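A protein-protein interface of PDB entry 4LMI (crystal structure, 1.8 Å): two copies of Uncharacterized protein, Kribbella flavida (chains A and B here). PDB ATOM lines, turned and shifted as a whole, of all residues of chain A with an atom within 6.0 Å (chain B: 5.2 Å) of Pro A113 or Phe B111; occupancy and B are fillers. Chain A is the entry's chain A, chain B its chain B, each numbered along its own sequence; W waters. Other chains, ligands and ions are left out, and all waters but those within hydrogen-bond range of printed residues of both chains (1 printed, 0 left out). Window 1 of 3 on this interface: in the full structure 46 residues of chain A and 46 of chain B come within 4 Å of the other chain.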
ATOM      1  N   GLN A  43     -10.148 -26.752  -2.962  1.00  0.00           N
ATOM      2  CA  GLN A  43      -8.923 -25.951  -2.820  1.00  0.00           C
ATOM      3  C   GLN A  43      -8.027 -25.965  -4.060  1.00  0.00           C
ATOM      4  O   GLN A  43      -7.304 -25.003  -4.320  1.00  0.00           O
ATOM      5  CB  GLN A  43      -8.104 -26.425  -1.625  1.00  0.00           C
ATOM      6  CG  GLN A  43      -8.654 -26.027  -0.266  1.00  0.00           C
ATOM      7  CD  GLN A  43      -8.057 -26.873   0.842  1.00  0.00           C
ATOM      8  OE1 GLN A  43      -8.476 -28.014   1.057  1.00  0.00           O
ATOM      9  NE2 GLN A  43      -7.069 -26.325   1.542  1.00  0.00           N
ATOM     10  N   ARG A  71     -14.068 -36.930  14.135  1.00  0.00           N
ATOM     11  CA  ARG A  71     -15.487 -36.566  14.247  1.00  0.00           C
ATOM     12  C   ARG A  71     -16.249 -37.187  13.095  1.00  0.00           C
ATOM     13  O   ARG A  71     -15.751 -37.252  11.971  1.00  0.00           O
ATOM     14  CB  ARG A  71     -15.714 -35.057  14.185  1.00  0.00           C
ATOM     15  CG  ARG A  71     -14.969 -34.199  15.191  1.00  0.00           C
ATOM     16  CD  ARG A  71     -15.216 -32.733  14.865  1.00  0.00           C
ATOM     17  NE  ARG A  71     -14.413 -31.836  15.688  1.00  0.00           N
ATOM     18  CZ  ARG A  71     -13.133 -31.545  15.459  1.00  0.00           C
ATOM     19  NH1 ARG A  71     -12.492 -32.087  14.430  1.00  0.00           N
ATOM     20  NH2 ARG A  71     -12.488 -30.718  16.272  1.00  0.00           N
ATOM     21  N   SER A  82     -14.187 -35.375  10.156  1.00  0.00           N
ATOM     22  CA  SER A  82     -12.808 -34.901  10.252  1.00  0.00           C
ATOM     23  C   SER A  82     -11.893 -36.095  10.475  1.00  0.00           C
ATOM     24  O   SER A  82     -12.282 -37.063  11.125  1.00  0.00           O
ATOM     25  CB  SER A  82     -12.638 -33.840  11.346  1.00  0.00           C
ATOM     26  OG  SER A  82     -13.070 -34.317  12.607  1.00  0.00           O
ATOM     27  N   VAL A  93      -4.712 -32.631   8.580  1.00  0.00           N
ATOM     28  CA  VAL A  93      -6.116 -32.787   8.954  1.00  0.00           C
ATOM     29  C   VAL A  93      -7.011 -32.650   7.724  1.00  0.00           C
ATOM     30  O   VAL A  93      -6.862 -31.718   6.931  1.00  0.00           O
ATOM     31  CB  VAL A  93      -6.544 -31.781  10.057  1.00  0.00           C
ATOM     32  CG1 VAL A  93      -8.033 -31.908  10.375  1.00  0.00           C
ATOM     33  CG2 VAL A  93      -5.736 -32.005  11.326  1.00  0.00           C
ATOM     34  N   GLY A  94      -7.936 -33.594   7.570  1.00  0.00           N
ATOM     35  CA  GLY A  94      -8.923 -33.536   6.498  1.00  0.00           C
ATOM     36  C   GLY A  94     -10.310 -33.330   7.060  1.00  0.00           C
ATOM     37  O   GLY A  94     -10.620 -33.809   8.156  1.00  0.00           O
ATOM     38  N   VAL A  95     -11.128 -32.586   6.320  1.00  0.00           N
ATOM     39  CA  VAL A  95     -12.548 -32.462   6.608  1.00  0.00           C
ATOM     40  C   VAL A  95     -13.300 -32.834   5.340  1.00  0.00           C
ATOM     41  O   VAL A  95     -13.078 -32.249   4.272  1.00  0.00           O
ATOM     42  CB  VAL A  95     -12.938 -31.052   7.092  1.00  0.00           C
ATOM     43  CG1 VAL A  95     -14.441 -30.980   7.333  1.00  0.00           C
ATOM     44  CG2 VAL A  95     -12.197 -30.711   8.374  1.00  0.00           C
ATOM     45  N   PHE A 111     -11.628 -31.285   2.145  1.00  0.00           N
ATOM     46  CA  PHE A 111     -10.827 -30.105   2.473  1.00  0.00           C
ATOM     47  C   PHE A 111      -9.616 -30.546   3.284  1.00  0.00           C
ATOM     48  O   PHE A 111      -9.729 -31.396   4.170  1.00  0.00           O
ATOM     49  CB  PHE A 111     -11.629 -29.077   3.275  1.00  0.00           C
ATOM     50  CG  PHE A 111     -12.807 -28.509   2.534  1.00  0.00           C
ATOM     51  CD1 PHE A 111     -12.662 -27.386   1.719  1.00  0.00           C
ATOM     52  CD2 PHE A 111     -14.067 -29.095   2.653  1.00  0.00           C
ATOM     53  CE1 PHE A 111     -13.755 -26.863   1.037  1.00  0.00           C
ATOM     54  CE2 PHE A 111     -15.162 -28.576   1.979  1.00  0.00           C
ATOM     55  CZ  PHE A 111     -15.005 -27.459   1.169  1.00  0.00           C
ATOM     56  N   TRP A 112      -8.462 -29.967   2.962  1.00  0.00           N
ATOM     57  CA  TRP A 112      -7.206 -30.261   3.633  1.00  0.00           C
ATOM     58  C   TRP A 112      -6.607 -28.946   4.052  1.00  0.00           C
ATOM     59  O   TRP A 112      -5.711 -28.419   3.376  1.00  0.00           O
ATOM     60  CB  TRP A 112      -6.289 -31.085   2.708  1.00  0.00           C
ATOM     61  CG  TRP A 112      -6.887 -32.452   2.497  1.00  0.00           C
ATOM     62  CD1 TRP A 112      -7.736 -32.861   1.469  1.00  0.00           C
ATOM     63  CD2 TRP A 112      -6.788 -33.613   3.397  1.00  0.00           C
ATOM     64  NE1 TRP A 112      -8.132 -34.171   1.652  1.00  0.00           N
ATOM     65  CE2 TRP A 112      -7.602 -34.677   2.788  1.00  0.00           C
ATOM     66  CE3 TRP A 112      -6.118 -33.874   4.589  1.00  0.00           C
ATOM     67  CZ2 TRP A 112      -7.719 -35.938   3.367  1.00  0.00           C
ATOM     68  CZ3 TRP A 112      -6.251 -35.145   5.166  1.00  0.00           C
ATOM     69  CH2 TRP A 112      -7.035 -36.152   4.568  1.00  0.00           C
ATOM     70  N   PRO A 113      -7.121 -28.368   5.160  1.00  0.00           N
ATOM     71  CA  PRO A 113      -6.658 -27.048   5.587  1.00  0.00           C
ATOM     72  C   PRO A 113      -5.221 -27.126   6.096  1.00  0.00           C
ATOM     73  O   PRO A 113      -4.918 -27.947   6.959  1.00  0.00           O
ATOM     74  CB  PRO A 113      -7.629 -26.670   6.724  1.00  0.00           C
ATOM     75  CG  PRO A 113      -8.735 -27.674   6.675  1.00  0.00           C
ATOM     76  CD  PRO A 113      -8.132 -28.911   6.088  1.00  0.00           C
ATOM     77  N   GLU A 114      -4.348 -26.289   5.540  1.00  0.00           N
ATOM     78  CA  GLU A 114      -2.923 -26.335   5.865  1.00  0.00           C
ATOM     79  C   GLU A 114      -2.620 -25.514   7.101  1.00  0.00           C
ATOM     80  O   GLU A 114      -3.211 -24.449   7.308  1.00  0.00           O
ATOM     81  CB  GLU A 114      -2.082 -25.811   4.696  1.00  0.00           C
ATOM     82  CG  GLU A 114      -2.299 -26.538   3.378  1.00  0.00           C
ATOM     83  CD  GLU A 114      -1.190 -26.269   2.377  1.00  0.00           C
ATOM     84  OE1 GLU A 114      -1.477 -25.703   1.304  1.00  0.00           O
ATOM     85  OE2 GLU A 114      -0.026 -26.618   2.666  1.00  0.00           O
ATOM     86  N   ALA A 115      -1.696 -26.005   7.921  1.00  0.00           N
ATOM     87  CA  ALA A 115      -1.193 -25.234   9.054  1.00  0.00           C
ATOM     88  C   ALA A 115      -0.574 -23.917   8.576  1.00  0.00           C
ATOM     89  O   ALA A 115       0.049 -23.864   7.510  1.00  0.00           O
ATOM     90  CB  ALA A 115      -0.178 -26.046   9.846  1.00  0.00           C
ATOM     91  N   ASP A 134      -7.383 -32.330  16.738  1.00  0.00           N
ATOM     92  CA  ASP A 134      -6.906 -32.164  15.370  1.00  0.00           C
ATOM     93  C   ASP A 134      -5.389 -32.010  15.355  1.00  0.00           C
ATOM     94  O   ASP A 134      -4.857 -31.039  15.906  1.00  0.00           O
ATOM     95  CB  ASP A 134      -7.621 -30.955  14.748  1.00  0.00           C
ATOM     96  CG  ASP A 134      -9.140 -31.055  14.878  1.00  0.00           C
ATOM     97  OD1 ASP A 134      -9.740 -31.904  14.191  1.00  0.00           O
ATOM     98  OD2 ASP A 134      -9.737 -30.297  15.672  1.00  0.00           O
ATOM     99  N   PHE A 136      -1.816 -31.422  13.745  1.00  0.00           N
ATOM    100  CA  PHE A 136      -0.909 -30.895  12.727  1.00  0.00           C
ATOM    101  C   PHE A 136       0.538 -31.103  13.166  1.00  0.00           C
ATOM    102  O   PHE A 136       0.805 -31.287  14.353  1.00  0.00           O
ATOM    103  CB  PHE A 136      -1.163 -29.404  12.504  1.00  0.00           C
ATOM    104  CG  PHE A 136      -2.410 -29.106  11.713  1.00  0.00           C
ATOM    105  CD1 PHE A 136      -2.387 -29.133  10.324  1.00  0.00           C
ATOM    106  CD2 PHE A 136      -3.598 -28.777  12.355  1.00  0.00           C
ATOM    107  CE1 PHE A 136      -3.526 -28.847   9.587  1.00  0.00           C
ATOM    108  CE2 PHE A 136      -4.744 -28.481  11.624  1.00  0.00           C
ATOM    109  CZ  PHE A 136      -4.708 -28.524  10.237  1.00  0.00           C
ATOM    110  N   PRO B  42      -7.210 -24.943  14.922  1.00  0.00           N
ATOM    111  CA  PRO B  42      -6.152 -25.960  14.909  1.00  0.00           C
ATOM    112  C   PRO B  42      -4.978 -25.668  13.974  1.00  0.00           C
ATOM    113  O   PRO B  42      -3.835 -26.010  14.307  1.00  0.00           O
ATOM    114  CB  PRO B  42      -6.893 -27.227  14.476  1.00  0.00           C
ATOM    115  CG  PRO B  42      -8.271 -27.025  15.024  1.00  0.00           C
ATOM    116  CD  PRO B  42      -8.549 -25.558  14.824  1.00  0.00           C
ATOM    117  N   GLN B  43      -5.251 -25.031  12.833  1.00  0.00           N
ATOM    118  CA  GLN B  43      -4.207 -24.703  11.852  1.00  0.00           C
ATOM    119  C   GLN B  43      -3.105 -23.819  12.440  1.00  0.00           C
ATOM    120  O   GLN B  43      -1.938 -23.933  12.061  1.00  0.00           O
ATOM    121  CB  GLN B  43      -4.811 -24.004  10.635  1.00  0.00           C
ATOM    122  CG  GLN B  43      -5.552 -24.899   9.655  1.00  0.00           C
ATOM    123  CD  GLN B  43      -6.448 -24.084   8.744  1.00  0.00           C
ATOM    124  OE1 GLN B  43      -7.562 -23.723   9.124  1.00  0.00           O
ATOM    125  NE2 GLN B  43      -5.961 -23.771   7.542  1.00  0.00           N
ATOM    126  N   VAL B  93     -12.837 -20.419   2.278  1.00  0.00           N
ATOM    127  CA  VAL B  93     -13.862 -21.329   2.782  1.00  0.00           C
ATOM    128  C   VAL B  93     -13.575 -21.613   4.254  1.00  0.00           C
ATOM    129  O   VAL B  93     -12.420 -21.773   4.660  1.00  0.00           O
ATOM    130  CB  VAL B  93     -13.957 -22.634   1.956  1.00  0.00           C
ATOM    131  CG1 VAL B  93     -14.839 -23.667   2.646  1.00  0.00           C
ATOM    132  CG2 VAL B  93     -14.495 -22.337   0.563  1.00  0.00           C
ATOM    133  N   GLY B  94     -14.629 -21.623   5.057  1.00  0.00           N
ATOM    134  CA  GLY B  94     -14.512 -22.037   6.445  1.00  0.00           C
ATOM    135  C   GLY B  94     -15.291 -23.311   6.656  1.00  0.00           C
ATOM    136  O   GLY B  94     -16.333 -23.512   6.041  1.00  0.00           O
ATOM    137  N   VAL B  95     -14.759 -24.185   7.499  1.00  0.00           N
ATOM    138  CA  VAL B  95     -15.491 -25.350   7.953  1.00  0.00           C
ATOM    139  C   VAL B  95     -15.392 -25.296   9.463  1.00  0.00           C
ATOM    140  O   VAL B  95     -14.294 -25.305  10.020  1.00  0.00           O
ATOM    141  CB  VAL B  95     -14.922 -26.682   7.428  1.00  0.00           C
ATOM    142  CG1 VAL B  95     -15.771 -27.835   7.944  1.00  0.00           C
ATOM    143  CG2 VAL B  95     -14.882 -26.701   5.905  1.00  0.00           C
ATOM    144  N   VAL B  96     -16.549 -25.220  10.109  1.00  0.00           N
ATOM    145  CA  VAL B  96     -16.629 -24.969  11.543  1.00  0.00           C
ATOM    146  C   VAL B  96     -17.394 -26.094  12.230  1.00  0.00           C
ATOM    147  O   VAL B  96     -18.505 -26.434  11.818  1.00  0.00           O
ATOM    148  CB  VAL B  96     -17.341 -23.626  11.828  1.00  0.00           C
ATOM    149  CG1 VAL B  96     -17.451 -23.379  13.328  1.00  0.00           C
ATOM    150  CG2 VAL B  96     -16.608 -22.470  11.157  1.00  0.00           C
ATOM    151  N   PHE B  97     -16.801 -26.663  13.278  1.00  0.00           N
ATOM    152  CA  PHE B  97     -17.494 -27.647  14.103  1.00  0.00           C
ATOM    153  C   PHE B  97     -17.960 -26.994  15.385  1.00  0.00           C
ATOM    154  O   PHE B  97     -17.175 -26.339  16.074  1.00  0.00           O
ATOM    155  CB  PHE B  97     -16.604 -28.850  14.412  1.00  0.00           C
ATOM    156  CG  PHE B  97     -16.272 -29.678  13.200  1.00  0.00           C
ATOM    157  CD1 PHE B  97     -17.149 -30.663  12.749  1.00  0.00           C
ATOM    158  CD2 PHE B  97     -15.087 -29.467  12.501  1.00  0.00           C
ATOM    159  CE1 PHE B  97     -16.846 -31.423  11.630  1.00  0.00           C
ATOM    160  CE2 PHE B  97     -14.776 -30.227  11.378  1.00  0.00           C
ATOM    161  CZ  PHE B  97     -15.657 -31.205  10.941  1.00  0.00           C
ATOM    162  N   THR B 109     -14.710 -25.039  16.736  1.00  0.00           N
ATOM    163  CA  THR B 109     -13.427 -25.378  16.126  1.00  0.00           C
ATOM    164  C   THR B 109     -13.482 -24.958  14.666  1.00  0.00           C
ATOM    165  O   THR B 109     -14.277 -25.498  13.893  1.00  0.00           O
ATOM    166  CB  THR B 109     -13.095 -26.879  16.289  1.00  0.00           C
ATOM    167  OG1 THR B 109     -13.080 -27.201  17.684  1.00  0.00           O
ATOM    168  CG2 THR B 109     -11.727 -27.213  15.709  1.00  0.00           C
ATOM    169  N   ASP B 110     -12.644 -23.975  14.326  1.00  0.00           N
ATOM    170  CA  ASP B 110     -12.617 -23.325  13.013  1.00  0.00           C
ATOM    171  C   ASP B 110     -11.505 -23.904  12.160  1.00  0.00           C
ATOM    172  O   ASP B 110     -10.368 -24.029  12.629  1.00  0.00           O
ATOM    173  CB  ASP B 110     -12.297 -21.831  13.177  1.00  0.00           C
ATOM    174  CG  ASP B 110     -13.533 -20.941  13.304  1.00  0.00           C
ATOM    175  OD1 ASP B 110     -14.629 -21.412  13.675  1.00  0.00           O
ATOM    176  OD2 ASP B 110     -13.380 -19.722  13.050  1.00  0.00           O
ATOM    177  N   PHE B 111     -11.835 -24.234  10.911  1.00  0.00           N
ATOM    178  CA  PHE B 111     -10.851 -24.518   9.869  1.00  0.00           C
ATOM    179  C   PHE B 111     -11.045 -23.522   8.736  1.00  0.00           C
ATOM    180  O   PHE B 111     -12.182 -23.236   8.347  1.00  0.00           O
ATOM    181  CB  PHE B 111     -11.028 -25.937   9.319  1.00  0.00           C
ATOM    182  CG  PHE B 111     -10.723 -27.015  10.315  1.00  0.00           C
ATOM    183  CD1 PHE B 111      -9.407 -27.433  10.523  1.00  0.00           C
ATOM    184  CD2 PHE B 111     -11.749 -27.623  11.041  1.00  0.00           C
ATOM    185  CE1 PHE B 111      -9.117 -28.433  11.441  1.00  0.00           C
ATOM    186  CE2 PHE B 111     -11.464 -28.626  11.961  1.00  0.00           C
ATOM    187  CZ  PHE B 111     -10.145 -29.029  12.160  1.00  0.00           C
ATOM    188  N   TRP B 112      -9.938 -22.999   8.211  1.00  0.00           N
ATOM    189  CA  TRP B 112      -9.986 -22.055   7.095  1.00  0.00           C
ATOM    190  C   TRP B 112      -9.115 -22.525   5.966  1.00  0.00           C
ATOM    191  O   TRP B 112      -8.012 -22.012   5.781  1.00  0.00           O
ATOM    192  CB  TRP B 112      -9.611 -20.652   7.570  1.00  0.00           C
ATOM    193  CG  TRP B 112     -10.616 -20.159   8.575  1.00  0.00           C
ATOM    194  CD1 TRP B 112     -10.507 -20.153   9.963  1.00  0.00           C
ATOM    195  CD2 TRP B 112     -11.963 -19.655   8.293  1.00  0.00           C
ATOM    196  NE1 TRP B 112     -11.656 -19.666  10.540  1.00  0.00           N
ATOM    197  CE2 TRP B 112     -12.569 -19.351   9.595  1.00  0.00           C
ATOM    198  CE3 TRP B 112     -12.697 -19.416   7.135  1.00  0.00           C
ATOM    199  CZ2 TRP B 112     -13.852 -18.829   9.706  1.00  0.00           C
ATOM    200  CZ3 TRP B 112     -13.991 -18.898   7.261  1.00  0.00           C
ATOM    201  CH2 TRP B 112     -14.552 -18.612   8.517  1.00  0.00           C
ATOM    202  N   PRO B 113      -9.592 -23.533   5.205  1.00  0.00           N
ATOM    203  CA  PRO B 113      -8.788 -24.040   4.098  1.00  0.00           C
ATOM    204  C   PRO B 113      -8.612 -22.969   3.037  1.00  0.00           C
ATOM    205  O   PRO B 113      -9.543 -22.200   2.771  1.00  0.00           O
ATOM    206  CB  PRO B 113      -9.623 -25.207   3.552  1.00  0.00           C
ATOM    207  CG  PRO B 113     -11.016 -24.958   4.036  1.00  0.00           C
ATOM    208  CD  PRO B 113     -10.846 -24.293   5.365  1.00  0.00           C
HETATM  209  O   HOH W   1      -4.484 -22.228   5.249  1.00  0.00           O
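The side-chain amide nitrogen (NE2) of Gln B43 sits at hydrogen-bond distance from the backbone carbonyl oxygen (O) of Glu A114, 2.8 Å away.
Hydrophobic or aromatic side chains of chain B within 4 Å of the printed part of chain A: Pro B42, Val B93, Val B95, Phe B97, Phe B111 and Pro B113.
Of the printed residues of chain B, Arg A71 touches Phe B97 (3.5 Å) and Thr B109 (3.6 Å).
Ser A82 touches none of the printed residues of chain B.
Of the printed residues of chain B, Val A93 touches Phe B111.
Pro A113 touches just these residues of chain B: Gln B43 (3.4 Å), Phe B111 (3.9 Å) and Pro B113 (3.9 Å).
Printed residues of chain A within 4 Å of Pro B42: Asp A134 (3.6 Å) and Phe A136 (3.4 Å).
Of the printed residues of chain A, Val B93 touches Phe A111 (3.7 Å).
Of the printed residues of chain A, Thr B109 touches Arg A71 (3.6 Å) and Asp A134 (3.7 Å).
Of chain A, only Val A93 (3.8 Å), Pro A113 (3.9 Å) and Asp A134 (3.5 Å) come within 4 Å of Phe B111.
Trp B112 touches none of the printed residues of chain A.
The nearest residue of chain A that does not touch Phe B111 is Val A95 (4.1 Å).
The nearest printed residue of chain A that does not touch Phe B97 is Ser A82 (4.03 Å).
Among the printed residues, pairs that only touch across the chains: Gln A43 with Pro B113, Arg A71 with Phe B97, Arg A71 with Thr B109, Val A93 with Phe B111, Val A95 with Val B95, Val A95 with Phe B97, Phe A111 with Val B93, Phe A111 with Pro B113, Pro A113 with Gln B43, Pro A113 with Phe B111, Pro A113 with Pro B113, Ala A115 with Gln B43, Asp A134 with Pro B42, Asp A134 with Thr B109, Asp A134 with Phe B111, Phe A136 with Pro B42 and Phe A136 with Gln B43.
Water W1 lies within hydrogen-bond range of the side-chain amide nitrogen (NE2) of Gln B43 (3.1 Å) and the backbone carbonyl oxygen (O) of Glu A114 (3.3 Å).
Gln A43 touches Pro B113, and with the chains exchanged Pro A113 touches Gln B43.
Val A93 touches Phe B111, and with the chains exchanged Phe A111 touches Val B93.
Phe A111 touches Pro B113, and with the chains exchanged Pro A113 touches Phe B111.
Pro A113 touches its own counterpart, Pro B113.
Positions printed for both chains: 43, 93, 94, 95, 111, 112 and 113.
NH1 of Arg A71 lies within salt-bridge range of OD1 of Asp A134.
The backbone carbonyl oxygen of Val A95 sits at hydrogen-bond distance from the backbone NH of Phe A111 (2.7 Å).
The backbone carbonyl oxygen of Thr B109 sits at hydrogen-bond distance from the backbone NH of Phe B97 (2.8 Å).
O of Val B95 lies within hydrogen-bond range of N of Phe B111 (2.8 Å).
The backbone NH of Trp B112 lies within hydrogen-bond range of the side-chain amide oxygen of Gln B43, at 2.6 Å.
The guanidinium group (NH1) of Arg A71 lies within hydrogen-bond range of the side-chain hydroxyl (OG) of Ser A82, 2.9 Å away.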
